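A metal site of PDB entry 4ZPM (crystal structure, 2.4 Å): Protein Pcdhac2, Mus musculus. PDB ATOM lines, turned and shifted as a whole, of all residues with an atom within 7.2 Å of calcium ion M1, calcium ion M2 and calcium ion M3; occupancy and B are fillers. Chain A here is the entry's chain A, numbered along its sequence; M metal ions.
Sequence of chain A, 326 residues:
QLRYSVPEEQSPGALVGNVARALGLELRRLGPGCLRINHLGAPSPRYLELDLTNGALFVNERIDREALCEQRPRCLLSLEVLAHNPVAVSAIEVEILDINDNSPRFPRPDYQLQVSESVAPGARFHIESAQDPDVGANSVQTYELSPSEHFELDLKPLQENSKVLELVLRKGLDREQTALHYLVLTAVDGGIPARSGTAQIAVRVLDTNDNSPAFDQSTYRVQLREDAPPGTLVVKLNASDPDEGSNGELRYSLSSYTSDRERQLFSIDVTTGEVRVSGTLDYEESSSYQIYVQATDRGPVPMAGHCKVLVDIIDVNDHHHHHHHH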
ATOM      1  N   GLU A   8      15.328  10.894 -15.174  1.00  0.00           N
ATOM      2  CA  GLU A   8      16.309   9.884 -14.800  1.00  0.00           C
ATOM      3  C   GLU A   8      16.160   9.465 -13.328  1.00  0.00           C
ATOM      4  O   GLU A   8      15.512  10.163 -12.543  1.00  0.00           O
ATOM      5  CB  GLU A   8      17.724  10.400 -15.056  1.00  0.00           C
ATOM      6  CG  GLU A   8      18.118  11.539 -14.135  1.00  0.00           C
ATOM      7  CD  GLU A   8      19.548  12.005 -14.334  1.00  0.00           C
ATOM      8  OE1 GLU A   8      20.466  11.152 -14.323  1.00  0.00           O
ATOM      9  OE2 GLU A   8      19.756  13.230 -14.497  1.00  0.00           O
ATOM     10  N   GLU A   9      16.741   8.326 -12.996  1.00  0.00           N
ATOM     11  CA  GLU A   9      16.913   7.877 -11.607  1.00  0.00           C
ATOM     12  C   GLU A   9      15.612   7.571 -10.860  1.00  0.00           C
ATOM     13  O   GLU A   9      15.614   7.516  -9.629  1.00  0.00           O
ATOM     14  CB  GLU A   9      17.702   8.942 -10.816  1.00  0.00           C
ATOM     15  CG  GLU A   9      19.069   9.284 -11.400  1.00  0.00           C
ATOM     16  CD  GLU A   9      20.095   8.173 -11.226  1.00  0.00           C
ATOM     17  OE1 GLU A   9      19.782   7.174 -10.544  1.00  0.00           O
ATOM     18  OE2 GLU A   9      21.204   8.307 -11.787  1.00  0.00           O
ATOM     19  N   ARG A  62      17.435   1.229 -13.066  1.00  0.00           N
ATOM     20  CA  ARG A  62      17.942   2.572 -12.816  1.00  0.00           C
ATOM     21  C   ARG A  62      18.473   3.183 -14.102  1.00  0.00           C
ATOM     22  O   ARG A  62      19.342   2.612 -14.774  1.00  0.00           O
ATOM     23  CB  ARG A  62      19.042   2.550 -11.747  1.00  0.00           C
ATOM     24  CG  ARG A  62      19.850   3.849 -11.678  1.00  0.00           C
ATOM     25  CD  ARG A  62      21.086   3.677 -10.808  1.00  0.00           C
ATOM     26  NE  ARG A  62      21.722   4.953 -10.504  1.00  0.00           N
ATOM     27  CZ  ARG A  62      22.902   5.333 -10.992  1.00  0.00           C
ATOM     28  NH1 ARG A  62      23.576   4.531 -11.804  1.00  0.00           N
ATOM     29  NH2 ARG A  62      23.403   6.521 -10.669  1.00  0.00           N
ATOM     30  N   ILE A  63      17.955   4.354 -14.452  1.00  0.00           N
ATOM     31  CA  ILE A  63      18.372   5.073 -15.646  1.00  0.00           C
ATOM     32  C   ILE A  63      19.181   6.302 -15.264  1.00  0.00           C
ATOM     33  O   ILE A  63      18.615   7.289 -14.797  1.00  0.00           O
ATOM     34  CB  ILE A  63      17.163   5.483 -16.501  1.00  0.00           C
ATOM     35  CG1 ILE A  63      16.254   4.278 -16.780  1.00  0.00           C
ATOM     36  CG2 ILE A  63      17.616   6.143 -17.800  1.00  0.00           C
ATOM     37  CD1 ILE A  63      15.136   4.569 -17.754  1.00  0.00           C
ATOM     38  N   ASP A  64      20.495   6.251 -15.446  1.00  0.00           N
ATOM     39  CA  ASP A  64      21.383   7.384 -15.125  1.00  0.00           C
ATOM     40  C   ASP A  64      21.776   8.144 -16.384  1.00  0.00           C
ATOM     41  O   ASP A  64      22.592   7.664 -17.178  1.00  0.00           O
ATOM     42  CB  ASP A  64      22.634   6.892 -14.392  1.00  0.00           C
ATOM     43  CG  ASP A  64      23.660   7.998 -14.146  1.00  0.00           C
ATOM     44  OD1 ASP A  64      23.260   9.163 -13.975  1.00  0.00           O
ATOM     45  OD2 ASP A  64      24.873   7.687 -14.114  1.00  0.00           O
ATOM     46  N   ARG A  65      21.197   9.326 -16.561  1.00  0.00           N
ATOM     47  CA  ARG A  65      21.446  10.132 -17.759  1.00  0.00           C
ATOM     48  C   ARG A  65      22.912  10.513 -17.908  1.00  0.00           C
ATOM     49  O   ARG A  65      23.425  10.591 -19.028  1.00  0.00           O
ATOM     50  CB  ARG A  65      20.588  11.398 -17.731  1.00  0.00           C
ATOM     51  CG  ARG A  65      20.566  12.138 -19.067  1.00  0.00           C
ATOM     52  CD  ARG A  65      20.514  13.645 -18.871  1.00  0.00           C
ATOM     53  NE  ARG A  65      21.666  14.135 -18.120  1.00  0.00           N
ATOM     54  CZ  ARG A  65      22.869  14.337 -18.645  1.00  0.00           C
ATOM     55  NH1 ARG A  65      23.077  14.088 -19.935  1.00  0.00           N
ATOM     56  NH2 ARG A  65      23.871  14.780 -17.890  1.00  0.00           N
ATOM     57  N   GLU A  66      23.594  10.733 -16.791  1.00  0.00           N
ATOM     58  CA  GLU A  66      25.002  11.096 -16.814  1.00  0.00           C
ATOM     59  C   GLU A  66      25.856   9.998 -17.432  1.00  0.00           C
ATOM     60  O   GLU A  66      26.750  10.265 -18.233  1.00  0.00           O
ATOM     61  CB  GLU A  66      25.509  11.437 -15.412  1.00  0.00           C
ATOM     62  CG  GLU A  66      25.221  12.876 -14.962  1.00  0.00           C
ATOM     63  CD  GLU A  66      23.760  13.130 -14.669  1.00  0.00           C
ATOM     64  OE1 GLU A  66      23.118  13.922 -15.394  1.00  0.00           O
ATOM     65  OE2 GLU A  66      23.237  12.553 -13.692  1.00  0.00           O
ATOM     66  N   ALA A  67      25.587   8.747 -17.060  1.00  0.00           N
ATOM     67  CA  ALA A  67      26.315   7.616 -17.616  1.00  0.00           C
ATOM     68  C   ALA A  67      25.963   7.392 -19.083  1.00  0.00           C
ATOM     69  O   ALA A  67      26.830   7.059 -19.890  1.00  0.00           O
ATOM     70  CB  ALA A  67      26.046   6.362 -16.810  1.00  0.00           C
ATOM     71  N   LEU A  97      14.941  12.861 -19.141  1.00  0.00           N
ATOM     72  CA  LEU A  97      15.094  14.206 -18.600  1.00  0.00           C
ATOM     73  C   LEU A  97      16.180  14.227 -17.536  1.00  0.00           C
ATOM     74  O   LEU A  97      16.359  13.264 -16.804  1.00  0.00           O
ATOM     75  CB  LEU A  97      13.773  14.708 -18.006  1.00  0.00           C
ATOM     76  CG  LEU A  97      12.539  14.655 -18.905  1.00  0.00           C
ATOM     77  CD1 LEU A  97      11.318  15.169 -18.166  1.00  0.00           C
ATOM     78  CD2 LEU A  97      12.776  15.443 -20.181  1.00  0.00           C
ATOM     79  N   ASP A  98      16.920  15.331 -17.487  1.00  0.00           N
ATOM     80  CA  ASP A  98      17.963  15.472 -16.489  1.00  0.00           C
ATOM     81  C   ASP A  98      17.422  16.042 -15.186  1.00  0.00           C
ATOM     82  O   ASP A  98      16.626  16.971 -15.205  1.00  0.00           O
ATOM     83  CB  ASP A  98      19.095  16.361 -17.016  1.00  0.00           C
ATOM     84  CG  ASP A  98      20.144  16.652 -15.968  1.00  0.00           C
ATOM     85  OD1 ASP A  98      20.879  15.708 -15.600  1.00  0.00           O
ATOM     86  OD2 ASP A  98      20.245  17.812 -15.530  1.00  0.00           O
ATOM     87  N   ILE A  99      17.847  15.465 -14.075  1.00  0.00           N
ATOM     88  CA  ILE A  99      17.547  16.032 -12.764  1.00  0.00           C
ATOM     89  C   ILE A  99      18.834  16.546 -12.134  1.00  0.00           C
ATOM     90  O   ILE A  99      19.939  16.172 -12.553  1.00  0.00           O
ATOM     91  CB  ILE A  99      16.870  15.009 -11.827  1.00  0.00           C
ATOM     92  CG1 ILE A  99      17.851  13.901 -11.439  1.00  0.00           C
ATOM     93  CG2 ILE A  99      15.623  14.434 -12.481  1.00  0.00           C
ATOM     94  CD1 ILE A  99      17.260  12.864 -10.495  1.00  0.00           C
ATOM     95  N   ASN A 100      18.695  17.410 -11.136  1.00  0.00           N
ATOM     96  CA  ASN A 100      19.851  17.996 -10.469  1.00  0.00           C
ATOM     97  C   ASN A 100      20.397  17.116  -9.363  1.00  0.00           C
ATOM     98  O   ASN A 100      20.341  17.476  -8.187  1.00  0.00           O
ATOM     99  CB  ASN A 100      19.489  19.373  -9.906  1.00  0.00           C
ATOM    100  CG  ASN A 100      20.707  20.244  -9.687  1.00  0.00           C
ATOM    101  OD1 ASN A 100      21.674  20.153 -10.442  1.00  0.00           O
ATOM    102  ND2 ASN A 100      20.668  21.083  -8.660  1.00  0.00           N
ATOM    103  N   ASP A 101      20.929  15.950  -9.732  1.00  0.00           N
ATOM    104  CA  ASP A 101      21.411  14.997  -8.743  1.00  0.00           C
ATOM    105  C   ASP A 101      22.932  15.007  -8.631  1.00  0.00           C
ATOM    106  O   ASP A 101      23.535  14.091  -8.079  1.00  0.00           O
ATOM    107  CB  ASP A 101      20.905  13.579  -9.074  1.00  0.00           C
ATOM    108  CG  ASP A 101      21.288  13.140 -10.478  1.00  0.00           C
ATOM    109  OD1 ASP A 101      21.519  14.015 -11.341  1.00  0.00           O
ATOM    110  OD2 ASP A 101      21.329  11.913 -10.723  1.00  0.00           O
ATOM    111  N   ASN A 102      23.550  16.052  -9.164  1.00  0.00           N
ATOM    112  CA  ASN A 102      24.991  16.237  -9.031  1.00  0.00           C
ATOM    113  C   ASN A 102      25.338  17.662  -8.612  1.00  0.00           C
ATOM    114  O   ASN A 102      24.672  18.614  -9.015  1.00  0.00           O
ATOM    115  CB  ASN A 102      25.713  15.886 -10.334  1.00  0.00           C
ATOM    116  CG  ASN A 102      25.624  14.412 -10.668  1.00  0.00           C
ATOM    117  OD1 ASN A 102      26.464  13.617 -10.246  1.00  0.00           O
ATOM    118  ND2 ASN A 102      24.603  14.047 -11.424  1.00  0.00           N
ATOM    119  N   SER A 103      26.379  17.799  -7.796  1.00  0.00           N
ATOM    120  CA  SER A 103      26.830  19.105  -7.355  1.00  0.00           C
ATOM    121  C   SER A 103      28.062  19.565  -8.130  1.00  0.00           C
ATOM    122  O   SER A 103      28.844  18.732  -8.590  1.00  0.00           O
ATOM    123  CB  SER A 103      27.137  19.078  -5.850  1.00  0.00           C
ATOM    124  OG  SER A 103      25.949  19.065  -5.090  1.00  0.00           O
ATOM    125  N   PRO A 104      28.223  20.882  -8.293  1.00  0.00           N
ATOM    126  CA  PRO A 104      29.438  21.454  -8.881  1.00  0.00           C
ATOM    127  C   PRO A 104      30.692  21.053  -8.111  1.00  0.00           C
ATOM    128  O   PRO A 104      30.682  21.084  -6.881  1.00  0.00           O
ATOM    129  CB  PRO A 104      29.197  22.963  -8.787  1.00  0.00           C
ATOM    130  CG  PRO A 104      27.724  23.088  -8.850  1.00  0.00           C
ATOM    131  CD  PRO A 104      27.215  21.924  -8.044  1.00  0.00           C
ATOM    132  N   ASP A 132      30.248  20.417 -13.469  1.00  0.00           N
ATOM    133  CA  ASP A 132      28.990  19.803 -13.035  1.00  0.00           C
ATOM    134  C   ASP A 132      28.471  18.864 -14.120  1.00  0.00           C
ATOM    135  O   ASP A 132      28.081  19.296 -15.192  1.00  0.00           O
ATOM    136  CB  ASP A 132      27.937  20.876 -12.716  1.00  0.00           C
ATOM    137  CG  ASP A 132      26.737  20.321 -11.960  1.00  0.00           C
ATOM    138  OD1 ASP A 132      26.267  19.204 -12.274  1.00  0.00           O
ATOM    139  OD2 ASP A 132      26.251  21.007 -11.040  1.00  0.00           O
ATOM    140  N   PRO A 133      28.487  17.548 -13.825  1.00  0.00           N
ATOM    141  CA  PRO A 133      28.120  16.541 -14.827  1.00  0.00           C
ATOM    142  C   PRO A 133      26.662  16.629 -15.300  1.00  0.00           C
ATOM    143  O   PRO A 133      26.311  15.962 -16.270  1.00  0.00           O
ATOM    144  CB  PRO A 133      28.384  15.212 -14.098  1.00  0.00           C
ATOM    145  CG  PRO A 133      28.362  15.545 -12.647  1.00  0.00           C
ATOM    146  CD  PRO A 133      28.878  16.953 -12.538  1.00  0.00           C
ATOM    147  N   ASP A 134      25.839  17.440 -14.644  1.00  0.00           N
ATOM    148  CA  ASP A 134      24.476  17.664 -15.110  1.00  0.00           C
ATOM    149  C   ASP A 134      24.505  18.560 -16.350  1.00  0.00           C
ATOM    150  O   ASP A 134      25.569  18.999 -16.780  1.00  0.00           O
ATOM    151  CB  ASP A 134      23.599  18.292 -14.031  1.00  0.00           C
ATOM    152  CG  ASP A 134      23.391  17.385 -12.841  1.00  0.00           C
ATOM    153  OD1 ASP A 134      23.716  16.182 -12.932  1.00  0.00           O
ATOM    154  OD2 ASP A 134      22.906  17.874 -11.803  1.00  0.00           O
ATOM    155  N   VAL A 135      23.328  18.832 -16.914  1.00  0.00           N
ATOM    156  CA  VAL A 135      23.227  19.602 -18.149  1.00  0.00           C
ATOM    157  C   VAL A 135      22.194  20.706 -18.018  1.00  0.00           C
ATOM    158  O   VAL A 135      21.360  20.687 -17.113  1.00  0.00           O
ATOM    159  CB  VAL A 135      22.860  18.701 -19.358  1.00  0.00           C
ATOM    160  CG1 VAL A 135      24.007  17.747 -19.678  1.00  0.00           C
ATOM    161  CG2 VAL A 135      21.569  17.943 -19.084  1.00  0.00           C
ATOM    162  N   ALA A 137      20.231  23.968 -17.101  1.00  0.00           N
ATOM    163  CA  ALA A 137      20.151  24.769 -15.885  1.00  0.00           C
ATOM    164  C   ALA A 137      20.775  24.059 -14.685  1.00  0.00           C
ATOM    165  O   ALA A 137      21.258  24.697 -13.758  1.00  0.00           O
ATOM    166  CB  ALA A 137      18.707  25.124 -15.587  1.00  0.00           C
ATOM    167  N   ASN A 138      20.754  22.734 -14.710  1.00  0.00           N
ATOM    168  CA  ASN A 138      21.287  21.941 -13.605  1.00  0.00           C
ATOM    169  C   ASN A 138      22.815  21.984 -13.508  1.00  0.00           C
ATOM    170  O   ASN A 138      23.391  21.500 -12.529  1.00  0.00           O
ATOM    171  CB  ASN A 138      20.820  20.495 -13.722  1.00  0.00           C
ATOM    172  CG  ASN A 138      19.335  20.342 -13.482  1.00  0.00           C
ATOM    173  OD1 ASN A 138      18.712  21.140 -12.793  1.00  0.00           O
ATOM    174  ND2 ASN A 138      18.747  19.296 -14.063  1.00  0.00           N
ATOM    175  N   SER A 139      23.472  22.547 -14.511  1.00  0.00           N
ATOM    176  CA  SER A 139      24.919  22.672 -14.502  1.00  0.00           C
ATOM    177  C   SER A 139      25.352  23.991 -13.870  1.00  0.00           C
ATOM    178  O   SER A 139      24.510  24.799 -13.485  1.00  0.00           O
ATOM    179  CB  SER A 139      25.485  22.548 -15.929  1.00  0.00           C
ATOM    180  OG  SER A 139      26.868  22.248 -15.898  1.00  0.00           O
ATOM    181  N   VAL A 140      26.664  24.213 -13.787  1.00  0.00           N
ATOM    182  CA  VAL A 140      27.194  25.430 -13.156  1.00  0.00           C
ATOM    183  C   VAL A 140      26.733  26.709 -13.858  1.00  0.00           C
ATOM    184  O   VAL A 140      26.889  26.850 -15.069  1.00  0.00           O
ATOM    185  CB  VAL A 140      28.717  25.408 -13.120  1.00  0.00           C
ATOM    186  CG1 VAL A 140      29.262  26.693 -12.510  1.00  0.00           C
ATOM    187  CG2 VAL A 140      29.205  24.189 -12.347  1.00  0.00           C
ATOM    188  N   ASP A 189      24.863  25.829  -9.138  1.00  0.00           N
ATOM    189  CA  ASP A 189      24.076  25.487 -10.323  1.00  0.00           C
ATOM    190  C   ASP A 189      22.725  26.189 -10.282  1.00  0.00           C
ATOM    191  O   ASP A 189      22.404  26.874  -9.310  1.00  0.00           O
ATOM    192  CB  ASP A 189      23.909  23.966 -10.486  1.00  0.00           C
ATOM    193  CG  ASP A 189      23.180  23.291  -9.322  1.00  0.00           C
ATOM    194  OD1 ASP A 189      22.259  23.889  -8.711  1.00  0.00           O
ATOM    195  OD2 ASP A 189      23.525  22.128  -9.025  1.00  0.00           O
ATOM    196  N   GLY A 190      21.927  26.017 -11.329  1.00  0.00           N
ATOM    197  CA  GLY A 190      20.647  26.690 -11.438  1.00  0.00           C
ATOM    198  C   GLY A 190      19.457  25.826 -11.093  1.00  0.00           C
ATOM    199  O   GLY A 190      18.306  26.208 -11.330  1.00  0.00           O
ATOM    200  N   GLY A 191      19.722  24.651 -10.538  1.00  0.00           N
ATOM    201  CA  GLY A 191      18.665  23.775 -10.067  1.00  0.00           C
ATOM    202  C   GLY A 191      17.971  24.356  -8.849  1.00  0.00           C
ATOM    203  O   GLY A 191      18.524  25.222  -8.180  1.00  0.00           O
ATOM    204  N   ARG A 195      22.548  23.589  -5.853  1.00  0.00           N
ATOM    205  CA  ARG A 195      23.609  22.788  -5.249  1.00  0.00           C
ATOM    206  C   ARG A 195      24.952  23.492  -5.447  1.00  0.00           C
ATOM    207  O   ARG A 195      25.185  24.144  -6.471  1.00  0.00           O
ATOM    208  CB  ARG A 195      23.630  21.383  -5.842  1.00  0.00           C
ATOM    209  CG  ARG A 195      22.322  20.632  -5.618  1.00  0.00           C
ATOM    210  CD  ARG A 195      22.349  19.233  -6.222  1.00  0.00           C
ATOM    211  NE  ARG A 195      23.408  18.413  -5.656  1.00  0.00           N
ATOM    212  CZ  ARG A 195      23.320  17.098  -5.467  1.00  0.00           C
ATOM    213  NH1 ARG A 195      22.207  16.458  -5.805  1.00  0.00           N
ATOM    214  NH2 ARG A 195      24.337  16.430  -4.940  1.00  0.00           N
HETATM  215 CA    CA M   1      23.993  19.995 -10.731  1.00  0.00          CA
HETATM  216 CA    CA M   2      21.649  14.653 -13.591  1.00  0.00          CA
HETATM  217 CA    CA M   3      22.240  10.673 -12.588  1.00  0.00          CA
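OD1 of Asp 101 lies close to ND2 of Asn 102, 3.1 Å away. The side-chain carboxylate of Glu 66 lies close to the side-chain amide nitrogen of Asn 102. The guanidinium group (NH2) of Arg 65 lies close to the side-chain carboxylate (OE1) of Glu 66. The backbone carbonyl oxygen (O) of Asp 132 sits at hydrogen-bond distance from the side-chain hydroxyl (OG) of Ser 139 (3.3 Å). The backbone carbonyl oxygen (O) of Leu 97 is in hydrogen-bond range of the backbone NH (N) of Glu 8, 3.1 Å away. The guanidinium group (NE) of Arg 62 is in salt-bridge range of the side-chain carboxylate (OE1) of Glu 9, at 2.9 Å. The side-chain carboxylate (OD1) of Asp 189 sits at hydrogen-bond distance from the backbone NH (N) of Arg 195 (2.9 Å). The backbone NH (N) of Gly 191 is in hydrogen-bond range of the side-chain carboxylate (OD1) of Asp 189 (3.2 Å).
Calcium ion M3 is bound by the side-chain carboxylate (OD1) of Asp 64, the side-chain carboxylate (OE2) of Glu 66, the side-chain carboxylate (OD2) of Asp 101, the side-chain carboxylate (OE1) of Glu 8 and the side-chain carboxylate (OE2) of Glu 9.
Seven residues have an atom within 4 Å of calcium ion M2: Glu 8, Glu 66, Asp 98, Ile 99, Asp 101, Asn 102 and Asp 134. The nearest printed residue that does not touch calcium ion M2 is Arg 65 (4.6 Å).
Calcium ion M1 is bound by O of Asn 102 (2.3 Å), OD1 of Asn 100 (2.3 Å), O of Asn 138 (2.4 Å), OD2 of Asp 132 (2.5 Å), OD2 of Asp 134 (2.6 Å), OD2 of Asp 189 (2.8 Å) and OD1 of Asp 132 (2.9 Å).
Of the 28 residues printed, 6 come within 4 Å of calcium ion M1. The nearest printed residue that does not touch calcium ion M1 is Ser 103 (4.4 Å).
Calcium ion M2 is bound by OD1 of Asp 101 (2.3 Å), OD1 of Asp 98 (2.4 Å), OE1 of Glu 66 (2.4 Å), O of Ile 99 (2.5 Å), OE2 of Glu 8 (2.5 Å), OE2 of Glu 66 (2.6 Å) and OD1 of Asp 134 (2.7 Å).
Five residues have an atom within 4 Å of calcium ion M3: Glu 8, Glu 9, Asp 64, Glu 66 and Asp 101.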
